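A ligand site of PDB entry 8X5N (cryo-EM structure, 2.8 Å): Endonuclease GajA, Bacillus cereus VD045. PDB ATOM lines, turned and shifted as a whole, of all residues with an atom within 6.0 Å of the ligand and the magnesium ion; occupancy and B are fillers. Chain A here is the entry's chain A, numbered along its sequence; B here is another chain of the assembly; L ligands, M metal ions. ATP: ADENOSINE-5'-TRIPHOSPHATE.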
ATOM      1  N   PHE A  11     -23.949 -15.233   5.765  1.00  0.00           N
ATOM      2  CA  PHE A  11     -23.102 -15.776   6.818  1.00  0.00           C
ATOM      3  C   PHE A  11     -23.466 -15.047   8.123  1.00  0.00           C
ATOM      4  O   PHE A  11     -24.525 -14.417   8.199  1.00  0.00           O
ATOM      5  CB  PHE A  11     -21.633 -15.645   6.357  1.00  0.00           C
ATOM      6  CG  PHE A  11     -20.660 -16.568   7.062  1.00  0.00           C
ATOM      7  CD1 PHE A  11     -20.823 -17.954   7.019  1.00  0.00           C
ATOM      8  CD2 PHE A  11     -19.540 -16.031   7.695  1.00  0.00           C
ATOM      9  CE1 PHE A  11     -19.918 -18.796   7.671  1.00  0.00           C
ATOM     10  CE2 PHE A  11     -18.620 -16.857   8.340  1.00  0.00           C
ATOM     11  CZ  PHE A  11     -18.810 -18.241   8.323  1.00  0.00           C
ATOM     12  N   ARG A  12     -22.607 -15.147   9.161  1.00  0.00           N
ATOM     13  CA  ARG A  12     -22.908 -14.828  10.564  1.00  0.00           C
ATOM     14  C   ARG A  12     -23.316 -13.380  10.847  1.00  0.00           C
ATOM     15  O   ARG A  12     -24.492 -13.125  11.091  1.00  0.00           O
ATOM     16  CB  ARG A  12     -21.704 -15.191  11.415  1.00  0.00           C
ATOM     17  CG  ARG A  12     -21.263 -16.628  11.259  1.00  0.00           C
ATOM     18  CD  ARG A  12     -20.033 -16.897  12.087  1.00  0.00           C
ATOM     19  NE  ARG A  12     -19.597 -18.282  12.004  1.00  0.00           N
ATOM     20  CZ  ARG A  12     -18.605 -18.780  12.717  1.00  0.00           C
ATOM     21  NH1 ARG A  12     -17.947 -18.049  13.605  1.00  0.00           N
ATOM     22  NH2 ARG A  12     -18.272 -20.057  12.562  1.00  0.00           N
ATOM     23  N   ASN A  13     -22.406 -12.431  10.716  1.00  0.00           N
ATOM     24  CA  ASN A  13     -22.819 -11.028  10.770  1.00  0.00           C
ATOM     25  C   ASN A  13     -22.537 -10.290   9.469  1.00  0.00           C
ATOM     26  O   ASN A  13     -22.338  -9.072   9.474  1.00  0.00           O
ATOM     27  CB  ASN A  13     -22.178 -10.329  11.979  1.00  0.00           C
ATOM     28  CG  ASN A  13     -20.692 -10.564  12.083  1.00  0.00           C
ATOM     29  OD1 ASN A  13     -20.065 -11.169  11.230  1.00  0.00           O
ATOM     30  ND2 ASN A  13     -20.125 -10.116  13.189  1.00  0.00           N
ATOM     31  N   GLY A  29     -10.628  -3.076  12.899  1.00  0.00           N
ATOM     32  CA  GLY A  29     -11.925  -2.581  13.319  1.00  0.00           C
ATOM     33  C   GLY A  29     -12.063  -2.633  14.833  1.00  0.00           C
ATOM     34  O   GLY A  29     -11.086  -2.816  15.550  1.00  0.00           O
ATOM     35  N   MET A  30     -13.310  -2.522  15.275  1.00  0.00           N
ATOM     36  CA  MET A  30     -13.663  -2.441  16.692  1.00  0.00           C
ATOM     37  C   MET A  30     -13.715  -3.824  17.343  1.00  0.00           C
ATOM     38  O   MET A  30     -13.258  -4.830  16.789  1.00  0.00           O
ATOM     39  CB  MET A  30     -15.025  -1.761  16.841  1.00  0.00           C
ATOM     40  CG  MET A  30     -15.074  -0.297  16.486  1.00  0.00           C
ATOM     41  SD  MET A  30     -14.053   0.743  17.520  1.00  0.00           S
ATOM     42  CE  MET A  30     -14.966   0.640  19.067  1.00  0.00           C
ATOM     43  N   ASN A  31     -14.244  -3.871  18.562  1.00  0.00           N
ATOM     44  CA  ASN A  31     -14.534  -5.143  19.219  1.00  0.00           C
ATOM     45  C   ASN A  31     -15.961  -5.555  18.906  1.00  0.00           C
ATOM     46  O   ASN A  31     -16.837  -4.687  18.773  1.00  0.00           O
ATOM     47  CB  ASN A  31     -14.357  -5.005  20.736  1.00  0.00           C
ATOM     48  CG  ASN A  31     -12.908  -4.904  21.156  1.00  0.00           C
ATOM     49  OD1 ASN A  31     -12.558  -4.087  21.997  1.00  0.00           O
ATOM     50  ND2 ASN A  31     -12.059  -5.730  20.570  1.00  0.00           N
ATOM     51  N   ASP A  32     -16.178  -6.880  18.790  1.00  0.00           N
ATOM     52  CA  ASP A  32     -17.451  -7.553  18.505  1.00  0.00           C
ATOM     53  C   ASP A  32     -18.092  -7.079  17.195  1.00  0.00           C
ATOM     54  O   ASP A  32     -19.299  -6.809  17.121  1.00  0.00           O
ATOM     55  CB  ASP A  32     -18.455  -7.437  19.665  1.00  0.00           C
ATOM     56  CG  ASP A  32     -18.398  -8.608  20.606  1.00  0.00           C
ATOM     57  OD1 ASP A  32     -17.509  -9.467  20.444  1.00  0.00           O
ATOM     58  OD2 ASP A  32     -19.244  -8.684  21.521  1.00  0.00           O
ATOM     59  N   ILE A  33     -17.275  -6.973  16.155  1.00  0.00           N
ATOM     60  CA  ILE A  33     -17.737  -6.262  14.970  1.00  0.00           C
ATOM     61  C   ILE A  33     -17.610  -7.217  13.778  1.00  0.00           C
ATOM     62  O   ILE A  33     -18.235  -7.013  12.734  1.00  0.00           O
ATOM     63  CB  ILE A  33     -16.956  -4.940  14.815  1.00  0.00           C
ATOM     64  CG1 ILE A  33     -17.696  -3.963  13.907  1.00  0.00           C
ATOM     65  CG2 ILE A  33     -15.535  -5.165  14.287  1.00  0.00           C
ATOM     66  CD1 ILE A  33     -19.000  -3.506  14.512  1.00  0.00           C
ATOM     67  N   GLY A  34     -16.861  -8.304  13.958  1.00  0.00           N
ATOM     68  CA  GLY A  34     -16.797  -9.336  12.939  1.00  0.00           C
ATOM     69  C   GLY A  34     -15.496  -9.468  12.178  1.00  0.00           C
ATOM     70  O   GLY A  34     -15.514  -9.712  10.971  1.00  0.00           O
ATOM     71  N   LYS A  35     -14.366  -9.287  12.856  1.00  0.00           N
ATOM     72  CA  LYS A  35     -13.081  -9.475  12.193  1.00  0.00           C
ATOM     73  C   LYS A  35     -12.734 -10.953  12.063  1.00  0.00           C
ATOM     74  O   LYS A  35     -12.176 -11.367  11.042  1.00  0.00           O
ATOM     75  CB  LYS A  35     -11.985  -8.741  12.949  1.00  0.00           C
ATOM     76  CG  LYS A  35     -12.145  -7.233  12.982  1.00  0.00           C
ATOM     77  CD  LYS A  35     -10.889  -6.576  13.481  1.00  0.00           C
ATOM     78  CE  LYS A  35     -10.568  -6.974  14.904  1.00  0.00           C
ATOM     79  NZ  LYS A  35      -9.118  -6.849  15.206  1.00  0.00           N
ATOM     80  N   THR A  36     -13.059 -11.762  13.075  1.00  0.00           N
ATOM     81  CA  THR A  36     -12.682 -13.176  13.021  1.00  0.00           C
ATOM     82  C   THR A  36     -13.748 -14.004  12.308  1.00  0.00           C
ATOM     83  O   THR A  36     -13.529 -15.191  12.045  1.00  0.00           O
ATOM     84  CB  THR A  36     -12.419 -13.712  14.420  1.00  0.00           C
ATOM     85  OG1 THR A  36     -11.804 -14.999  14.334  1.00  0.00           O
ATOM     86  CG2 THR A  36     -13.709 -13.857  15.201  1.00  0.00           C
ATOM     87  N   ASN A  37     -14.895 -13.406  11.992  1.00  0.00           N
ATOM     88  CA  ASN A  37     -15.866 -14.072  11.135  1.00  0.00           C
ATOM     89  C   ASN A  37     -15.529 -13.875   9.657  1.00  0.00           C
ATOM     90  O   ASN A  37     -16.076 -14.576   8.803  1.00  0.00           O
ATOM     91  CB  ASN A  37     -17.273 -13.560  11.418  1.00  0.00           C
ATOM     92  CG  ASN A  37     -17.831 -14.102  12.718  1.00  0.00           C
ATOM     93  OD1 ASN A  37     -17.228 -14.957  13.361  1.00  0.00           O
ATOM     94  ND2 ASN A  37     -18.994 -13.602  13.099  1.00  0.00           N
ATOM     95  N   LYS A  57     -26.592 -24.227  13.264  1.00  0.00           N
ATOM     96  CA  LYS A  57     -27.666 -23.246  13.191  1.00  0.00           C
ATOM     97  C   LYS A  57     -27.120 -21.827  13.326  1.00  0.00           C
ATOM     98  O   LYS A  57     -27.644 -20.896  12.693  1.00  0.00           O
ATOM     99  CB  LYS A  57     -28.690 -23.533  14.298  1.00  0.00           C
ATOM    100  CG  LYS A  57     -29.976 -22.716  14.228  1.00  0.00           C
ATOM    101  CD  LYS A  57     -30.936 -23.073  15.345  1.00  0.00           C
ATOM    102  CE  LYS A  57     -32.085 -22.089  15.412  1.00  0.00           C
ATOM    103  NZ  LYS A  57     -32.919 -22.127  14.189  1.00  0.00           N
ATOM    104  N   SER A  58     -26.043 -21.652  14.089  1.00  0.00           N
ATOM    105  CA  SER A  58     -25.520 -20.343  14.447  1.00  0.00           C
ATOM    106  C   SER A  58     -24.768 -19.639  13.326  1.00  0.00           C
ATOM    107  O   SER A  58     -24.519 -18.443  13.429  1.00  0.00           O
ATOM    108  CB  SER A  58     -24.597 -20.483  15.656  1.00  0.00           C
ATOM    109  OG  SER A  58     -23.423 -21.201  15.314  1.00  0.00           O
ATOM    110  N   ASP A  59     -24.428 -20.347  12.250  1.00  0.00           N
ATOM    111  CA  ASP A  59     -23.665 -19.782  11.143  1.00  0.00           C
ATOM    112  C   ASP A  59     -24.517 -18.994  10.169  1.00  0.00           C
ATOM    113  O   ASP A  59     -23.969 -18.336   9.275  1.00  0.00           O
ATOM    114  CB  ASP A  59     -22.928 -20.892  10.406  1.00  0.00           C
ATOM    115  CG  ASP A  59     -21.790 -21.473  11.209  1.00  0.00           C
ATOM    116  OD1 ASP A  59     -20.802 -20.742  11.447  1.00  0.00           O
ATOM    117  OD2 ASP A  59     -21.864 -22.647  11.606  1.00  0.00           O
ATOM    118  N   TYR A  60     -25.843 -19.023  10.301  1.00  0.00           N
ATOM    119  CA  TYR A  60     -26.747 -18.331   9.398  1.00  0.00           C
ATOM    120  C   TYR A  60     -27.039 -16.942   9.959  1.00  0.00           C
ATOM    121  O   TYR A  60     -26.826 -16.674  11.141  1.00  0.00           O
ATOM    122  CB  TYR A  60     -28.048 -19.133   9.206  1.00  0.00           C
ATOM    123  CG  TYR A  60     -27.869 -20.387   8.372  1.00  0.00           C
ATOM    124  CD1 TYR A  60     -27.440 -21.593   8.952  1.00  0.00           C
ATOM    125  CD2 TYR A  60     -28.125 -20.370   6.998  1.00  0.00           C
ATOM    126  CE1 TYR A  60     -27.259 -22.736   8.179  1.00  0.00           C
ATOM    127  CE2 TYR A  60     -27.957 -21.514   6.207  1.00  0.00           C
ATOM    128  CZ  TYR A  60     -27.524 -22.690   6.823  1.00  0.00           C
ATOM    129  OH  TYR A  60     -27.348 -23.819   6.058  1.00  0.00           O
ATOM    130  N   HIS A  61     -27.513 -16.043   9.083  1.00  0.00           N
ATOM    131  CA  HIS A  61     -27.692 -14.641   9.442  1.00  0.00           C
ATOM    132  C   HIS A  61     -28.946 -14.469  10.289  1.00  0.00           C
ATOM    133  O   HIS A  61     -30.055 -14.712   9.816  1.00  0.00           O
ATOM    134  CB  HIS A  61     -27.794 -13.770   8.194  1.00  0.00           C
ATOM    135  CG  HIS A  61     -27.697 -12.303   8.484  1.00  0.00           C
ATOM    136  ND1 HIS A  61     -26.797 -11.785   9.394  1.00  0.00           N
ATOM    137  CD2 HIS A  61     -28.376 -11.252   7.985  1.00  0.00           C
ATOM    138  CE1 HIS A  61     -26.933 -10.473   9.440  1.00  0.00           C
ATOM    139  NE2 HIS A  61     -27.885 -10.125   8.602  1.00  0.00           N
ATOM    140  N   LYS A  62     -28.726 -14.053  11.556  1.00  0.00           N
ATOM    141  CA  LYS A  62     -29.731 -13.896  12.626  1.00  0.00           C
ATOM    142  C   LYS A  62     -30.493 -15.182  12.905  1.00  0.00           C
ATOM    143  O   LYS A  62     -31.693 -15.128  13.213  1.00  0.00           O
ATOM    144  CB  LYS A  62     -30.698 -12.726  12.360  1.00  0.00           C
ATOM    145  CG  LYS A  62     -30.017 -11.380  12.190  1.00  0.00           C
ATOM    146  CD  LYS A  62     -31.024 -10.301  11.856  1.00  0.00           C
ATOM    147  CE  LYS A  62     -30.335  -8.977  11.564  1.00  0.00           C
ATOM    148  NZ  LYS A  62     -29.702  -8.403  12.778  1.00  0.00           N
ATOM    149  N   HIS A  63     -29.776 -16.315  12.820  1.00  0.00           N
ATOM    150  CA  HIS A  63     -30.233 -17.701  13.087  1.00  0.00           C
ATOM    151  C   HIS A  63     -31.442 -18.085  12.235  1.00  0.00           C
ATOM    152  O   HIS A  63     -32.368 -18.742  12.707  1.00  0.00           O
ATOM    153  CB  HIS A  63     -30.515 -17.923  14.569  1.00  0.00           C
ATOM    154  CG  HIS A  63     -29.286 -18.070  15.415  1.00  0.00           C
ATOM    155  ND1 HIS A  63     -29.288 -18.752  16.617  1.00  0.00           N
ATOM    156  CD2 HIS A  63     -28.026 -17.602  15.254  1.00  0.00           C
ATOM    157  CE1 HIS A  63     -28.079 -18.718  17.141  1.00  0.00           C
ATOM    158  NE2 HIS A  63     -27.293 -18.019  16.337  1.00  0.00           N
ATOM    159  N   GLU A 288      -4.394 -14.499  13.102  1.00  0.00           N
ATOM    160  CA  GLU A 288      -5.402 -13.900  13.973  1.00  0.00           C
ATOM    161  C   GLU A 288      -4.715 -13.328  15.197  1.00  0.00           C
ATOM    162  O   GLU A 288      -4.263 -14.094  16.062  1.00  0.00           O
ATOM    163  CB  GLU A 288      -6.452 -14.938  14.357  1.00  0.00           C
ATOM    164  CG  GLU A 288      -7.523 -14.454  15.335  1.00  0.00           C
ATOM    165  CD  GLU A 288      -8.577 -13.587  14.699  1.00  0.00           C
ATOM    166  OE1 GLU A 288      -8.921 -13.837  13.529  1.00  0.00           O
ATOM    167  OE2 GLU A 288      -9.050 -12.645  15.363  1.00  0.00           O
ATOM    168  N   GLU A 289      -4.636 -11.986  15.265  1.00  0.00           N
ATOM    169  CA  GLU A 289      -4.123 -11.125  16.335  1.00  0.00           C
ATOM    170  C   GLU A 289      -2.712 -11.468  16.818  1.00  0.00           C
ATOM    171  O   GLU A 289      -2.561 -11.992  17.926  1.00  0.00           O
ATOM    172  CB  GLU A 289      -5.100 -11.131  17.512  1.00  0.00           C
ATOM    173  CG  GLU A 289      -6.209 -10.100  17.386  1.00  0.00           C
ATOM    174  CD  GLU A 289      -7.421 -10.430  18.238  1.00  0.00           C
ATOM    175  OE1 GLU A 289      -7.508 -11.579  18.716  1.00  0.00           O
ATOM    176  OE2 GLU A 289      -8.273  -9.539  18.439  1.00  0.00           O
ATOM    177  N   HIS A 320      -4.948  -5.428  16.290  1.00  0.00           N
ATOM    178  CA  HIS A 320      -5.366  -4.268  17.077  1.00  0.00           C
ATOM    179  C   HIS A 320      -4.237  -3.292  17.302  1.00  0.00           C
ATOM    180  O   HIS A 320      -4.449  -2.242  17.922  1.00  0.00           O
ATOM    181  CB  HIS A 320      -5.911  -4.701  18.446  1.00  0.00           C
ATOM    182  CG  HIS A 320      -7.342  -5.131  18.438  1.00  0.00           C
ATOM    183  ND1 HIS A 320      -8.379  -4.263  18.214  1.00  0.00           N
ATOM    184  CD2 HIS A 320      -7.911  -6.329  18.692  1.00  0.00           C
ATOM    185  CE1 HIS A 320      -9.528  -4.911  18.294  1.00  0.00           C
ATOM    186  NE2 HIS A 320      -9.265  -6.174  18.586  1.00  0.00           N
ATOM    187  N   GLY B 258     -18.449 -13.350  21.207  1.00  0.00           N
ATOM    188  CA  GLY B 258     -17.270 -12.845  20.546  1.00  0.00           C
ATOM    189  C   GLY B 258     -16.087 -12.679  21.477  1.00  0.00           C
ATOM    190  O   GLY B 258     -15.781 -13.572  22.272  1.00  0.00           O
ATOM    191  N   ASP B 259     -15.416 -11.534  21.389  1.00  0.00           N
ATOM    192  CA  ASP B 259     -14.292 -11.227  22.263  1.00  0.00           C
ATOM    193  C   ASP B 259     -14.291  -9.732  22.556  1.00  0.00           C
ATOM    194  O   ASP B 259     -15.013  -8.957  21.932  1.00  0.00           O
ATOM    195  CB  ASP B 259     -12.962 -11.662  21.648  1.00  0.00           C
ATOM    196  CG  ASP B 259     -11.986 -12.159  22.686  1.00  0.00           C
ATOM    197  OD1 ASP B 259     -11.967 -11.607  23.802  1.00  0.00           O
ATOM    198  OD2 ASP B 259     -11.232 -13.112  22.382  1.00  0.00           O
ATOM    199  N   GLY B 260     -13.504  -9.341  23.556  1.00  0.00           N
ATOM    200  CA  GLY B 260     -13.375  -7.933  23.902  1.00  0.00           C
ATOM    201  C   GLY B 260     -14.481  -7.378  24.781  1.00  0.00           C
ATOM    202  O   GLY B 260     -14.202  -6.863  25.871  1.00  0.00           O
ATOM    203  N   ARG B 261     -15.733  -7.440  24.312  1.00  0.00           N
ATOM    204  CA  ARG B 261     -16.880  -7.003  25.097  1.00  0.00           C
ATOM    205  C   ARG B 261     -17.162  -7.947  26.261  1.00  0.00           C
ATOM    206  O   ARG B 261     -17.704  -7.515  27.286  1.00  0.00           O
ATOM    207  CB  ARG B 261     -18.115  -6.913  24.190  1.00  0.00           C
ATOM    208  CG  ARG B 261     -18.038  -5.876  23.081  1.00  0.00           C
ATOM    209  CD  ARG B 261     -18.292  -4.471  23.580  1.00  0.00           C
ATOM    210  NE  ARG B 261     -18.446  -3.528  22.474  1.00  0.00           N
ATOM    211  CZ  ARG B 261     -17.495  -2.735  22.023  1.00  0.00           C
ATOM    212  NH1 ARG B 261     -16.289  -2.725  22.573  1.00  0.00           N
ATOM    213  NH2 ARG B 261     -17.754  -1.925  20.995  1.00  0.00           N
ATOM    214  N   SER B 293      -6.617  -8.643  22.736  1.00  0.00           N
ATOM    215  CA  SER B 293      -7.823  -8.613  21.877  1.00  0.00           C
ATOM    216  C   SER B 293      -8.785  -7.492  22.274  1.00  0.00           C
ATOM    217  O   SER B 293     -10.008  -7.664  22.256  1.00  0.00           O
ATOM    218  CB  SER B 293      -8.535  -9.969  21.847  1.00  0.00           C
ATOM    219  OG  SER B 293      -9.267 -10.178  23.045  1.00  0.00           O
ATOM    220  N   LEU B 294      -8.239  -6.333  22.614  1.00  0.00           N
ATOM    221  CA  LEU B 294      -9.034  -5.212  23.070  1.00  0.00           C
ATOM    222  C   LEU B 294      -8.602  -3.978  22.297  1.00  0.00           C
ATOM    223  O   LEU B 294      -7.402  -3.773  22.084  1.00  0.00           O
ATOM    224  CB  LEU B 294      -8.858  -5.011  24.585  1.00  0.00           C
ATOM    225  CG  LEU B 294      -9.675  -3.939  25.294  1.00  0.00           C
ATOM    226  CD1 LEU B 294     -11.125  -4.334  25.148  1.00  0.00           C
ATOM    227  CD2 LEU B 294      -9.283  -3.860  26.736  1.00  0.00           C
HETATM  228  PG  ATP L   1     -12.430  -8.674  18.855  1.00  0.00           P
HETATM  229  O1G ATP L   1     -11.612  -9.890  19.066  1.00  0.00           O
HETATM  230  O2G ATP L   1     -11.764  -7.626  17.987  1.00  0.00           O
HETATM  231  O3G ATP L   1     -12.892  -8.010  20.131  1.00  0.00           O
HETATM  232  PB  ATP L   1     -14.269  -9.456  16.640  1.00  0.00           P
HETATM  233  O1B ATP L   1     -14.312  -8.316  15.723  1.00  0.00           O
HETATM  234  O2B ATP L   1     -13.380 -10.627  16.216  1.00  0.00           O
HETATM  235  O3B ATP L   1     -13.779  -9.032  18.078  1.00  0.00           O
HETATM  236  PA  ATP L   1     -16.459 -11.445  16.807  1.00  0.00           P
HETATM  237  O1A ATP L   1     -15.757 -12.523  17.525  1.00  0.00           O
HETATM  238  O2A ATP L   1     -16.680 -11.701  15.323  1.00  0.00           O
HETATM  239  O3A ATP L   1     -15.717 -10.041  16.935  1.00  0.00           O
HETATM  240  O5' ATP L   1     -17.845 -11.149  17.491  1.00  0.00           O
HETATM  241  C5' ATP L   1     -19.057 -11.786  17.032  1.00  0.00           C
HETATM  242  C4' ATP L   1     -20.030 -10.703  16.628  1.00  0.00           C
HETATM  243  O4' ATP L   1     -20.803 -11.153  15.492  1.00  0.00           O
HETATM  244  C3' ATP L   1     -21.046 -10.310  17.685  1.00  0.00           C
HETATM  245  O3' ATP L   1     -21.453  -8.962  17.530  1.00  0.00           O
HETATM  246  C2' ATP L   1     -22.190 -11.277  17.400  1.00  0.00           C
HETATM  247  O2' ATP L   1     -23.445 -10.765  17.850  1.00  0.00           O
HETATM  248  C1' ATP L   1     -22.155 -11.347  15.879  1.00  0.00           C
HETATM  249  N9  ATP L   1     -22.608 -12.617  15.333  1.00  0.00           N
HETATM  250  C8  ATP L   1     -21.910 -13.798  15.293  1.00  0.00           C
HETATM  251  N7  ATP L   1     -22.571 -14.795  14.748  1.00  0.00           N
HETATM  252  C5  ATP L   1     -23.787 -14.235  14.411  1.00  0.00           C
HETATM  253  C6  ATP L   1     -24.952 -14.754  13.795  1.00  0.00           C
HETATM  254  N6  ATP L   1     -25.073 -16.017  13.398  1.00  0.00           N
HETATM  255  N1  ATP L   1     -26.003 -13.907  13.598  1.00  0.00           N
HETATM  256  C2  ATP L   1     -25.898 -12.629  13.995  1.00  0.00           C
HETATM  257  N3  ATP L   1     -24.852 -12.041  14.582  1.00  0.00           N
HETATM  258  C4  ATP L   1     -23.827 -12.895  14.764  1.00  0.00           C
HETATM  259 MG    MG M   1     -12.130 -11.979  17.227  1.00  0.00          MG
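O of Tyr 60 sits at hydrogen-bond distance from N6 of the ligand (2.9 Å).
The backbone carbonyl oxygen (O) of Ser 58 is in hydrogen-bond range of a nitrogen (N6) of the ligand.
A nitrogen (N1) of the ligand is in hydrogen-bond range of the backbone NH of Lys 62.
ND2 of Asn 13 sits at hydrogen-bond distance from O4' of the ligand (2.6 Å).
N of Ile 33 lies within hydrogen-bond range of O1B of the ligand (3.3 Å).
An oxygen (O1B) of the ligand sits at hydrogen-bond distance from the backbone NH of Gly 34, at 3.1 Å.
N of Asp 32 lies within hydrogen-bond range of O3B of the ligand (3.3 Å).
The backbone NH (N) of Lys 35 sits at hydrogen-bond distance from an oxygen (O1B) of the ligand (3.0 Å).
The backbone carbonyl oxygen (O) of Asp 259 of chain B lies close to an oxygen (O3G) of the ligand (2.9 Å).
A ring nitrogen (NE2) of His 320 sits at hydrogen-bond distance from an oxygen (O2G) of the ligand, at 3.0 Å.
The backbone carbonyl oxygen of Asp 32 sits at hydrogen-bond distance from an oxygen (O3') of the ligand, at 3.1 Å.
N of Thr 36 sits close to O2B of the ligand (3.4 Å).
An oxygen (O3G) of the ligand is in hydrogen-bond range of the side-chain amide nitrogen of Asn 31, 2.5 Å away.
NZ of Lys 35 lies within salt-bridge range of O2G of the ligand (3.9 Å).
N1 of the ligand lies close to O of Arg 12, 3.0 Å away.
O of Met 30 sits close to O2G of the ligand (3.4 Å).
The side-chain carboxylate of Glu 289 lies close to an oxygen (O1G) of the ligand (3.4 Å).
Residues that only touch the ligand: Asn 37 (3.7 Å), His 63 (3.8 Å), Gly 258 of chain B (3.4 Å), Gly 260 of chain B (3.7 Å) and Ser 293 of chain B (3.6 Å).
Hydrophobic or aromatic side chains that line the ligand: Ile 33, His 63 and His 320.
Of the 28 residues printed, 20 come within 4 Å of the ligand.
The nearest printed residue that does not touch the ligand is Asp 59 (4.4 Å).
The side-chain amide nitrogen (ND2) of Asn 31 sits at hydrogen-bond distance from the backbone carbonyl oxygen (O) of Ser 293 of chain B.
The guanidinium group (NH1) of Arg 12 lies within hydrogen-bond range of the side-chain amide oxygen (OD1) of Asn 37, at 3.2 Å.
ND2 of Asn 31 lies within hydrogen-bond range of NE2 of His 320, 3.5 Å away.
The backbone carbonyl oxygen (O) of Arg 12 is in hydrogen-bond range of a ring nitrogen (ND1) of His 61.
OG of Ser 293 of chain B sits at hydrogen-bond distance from OD1 of Asp 259 of chain B, at 3.1 Å.
ND2 of Asn 37 sits at hydrogen-bond distance from OD1 of Asn 13, at 3.2 Å.
The side-chain carboxylate (OD1) of Asp 32 sits at hydrogen-bond distance from the backbone NH (N) of Asp 259 of chain B (3.1 Å).
The side-chain carboxylate (OD1) of Asp 59 is in salt-bridge range of the guanidinium group (NE) of Arg 12 (2.8 Å).
The magnesium ion is bound by O2B of the ligand.
Slightly farther from the magnesium ion lies an oxygen (O1G) of the ligand (2.8 Å).
Merely in contact with the magnesium ion: Thr 36 and Glu 288.
Of the 28 residues printed, 2 come within 4 Å of the magnesium ion.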
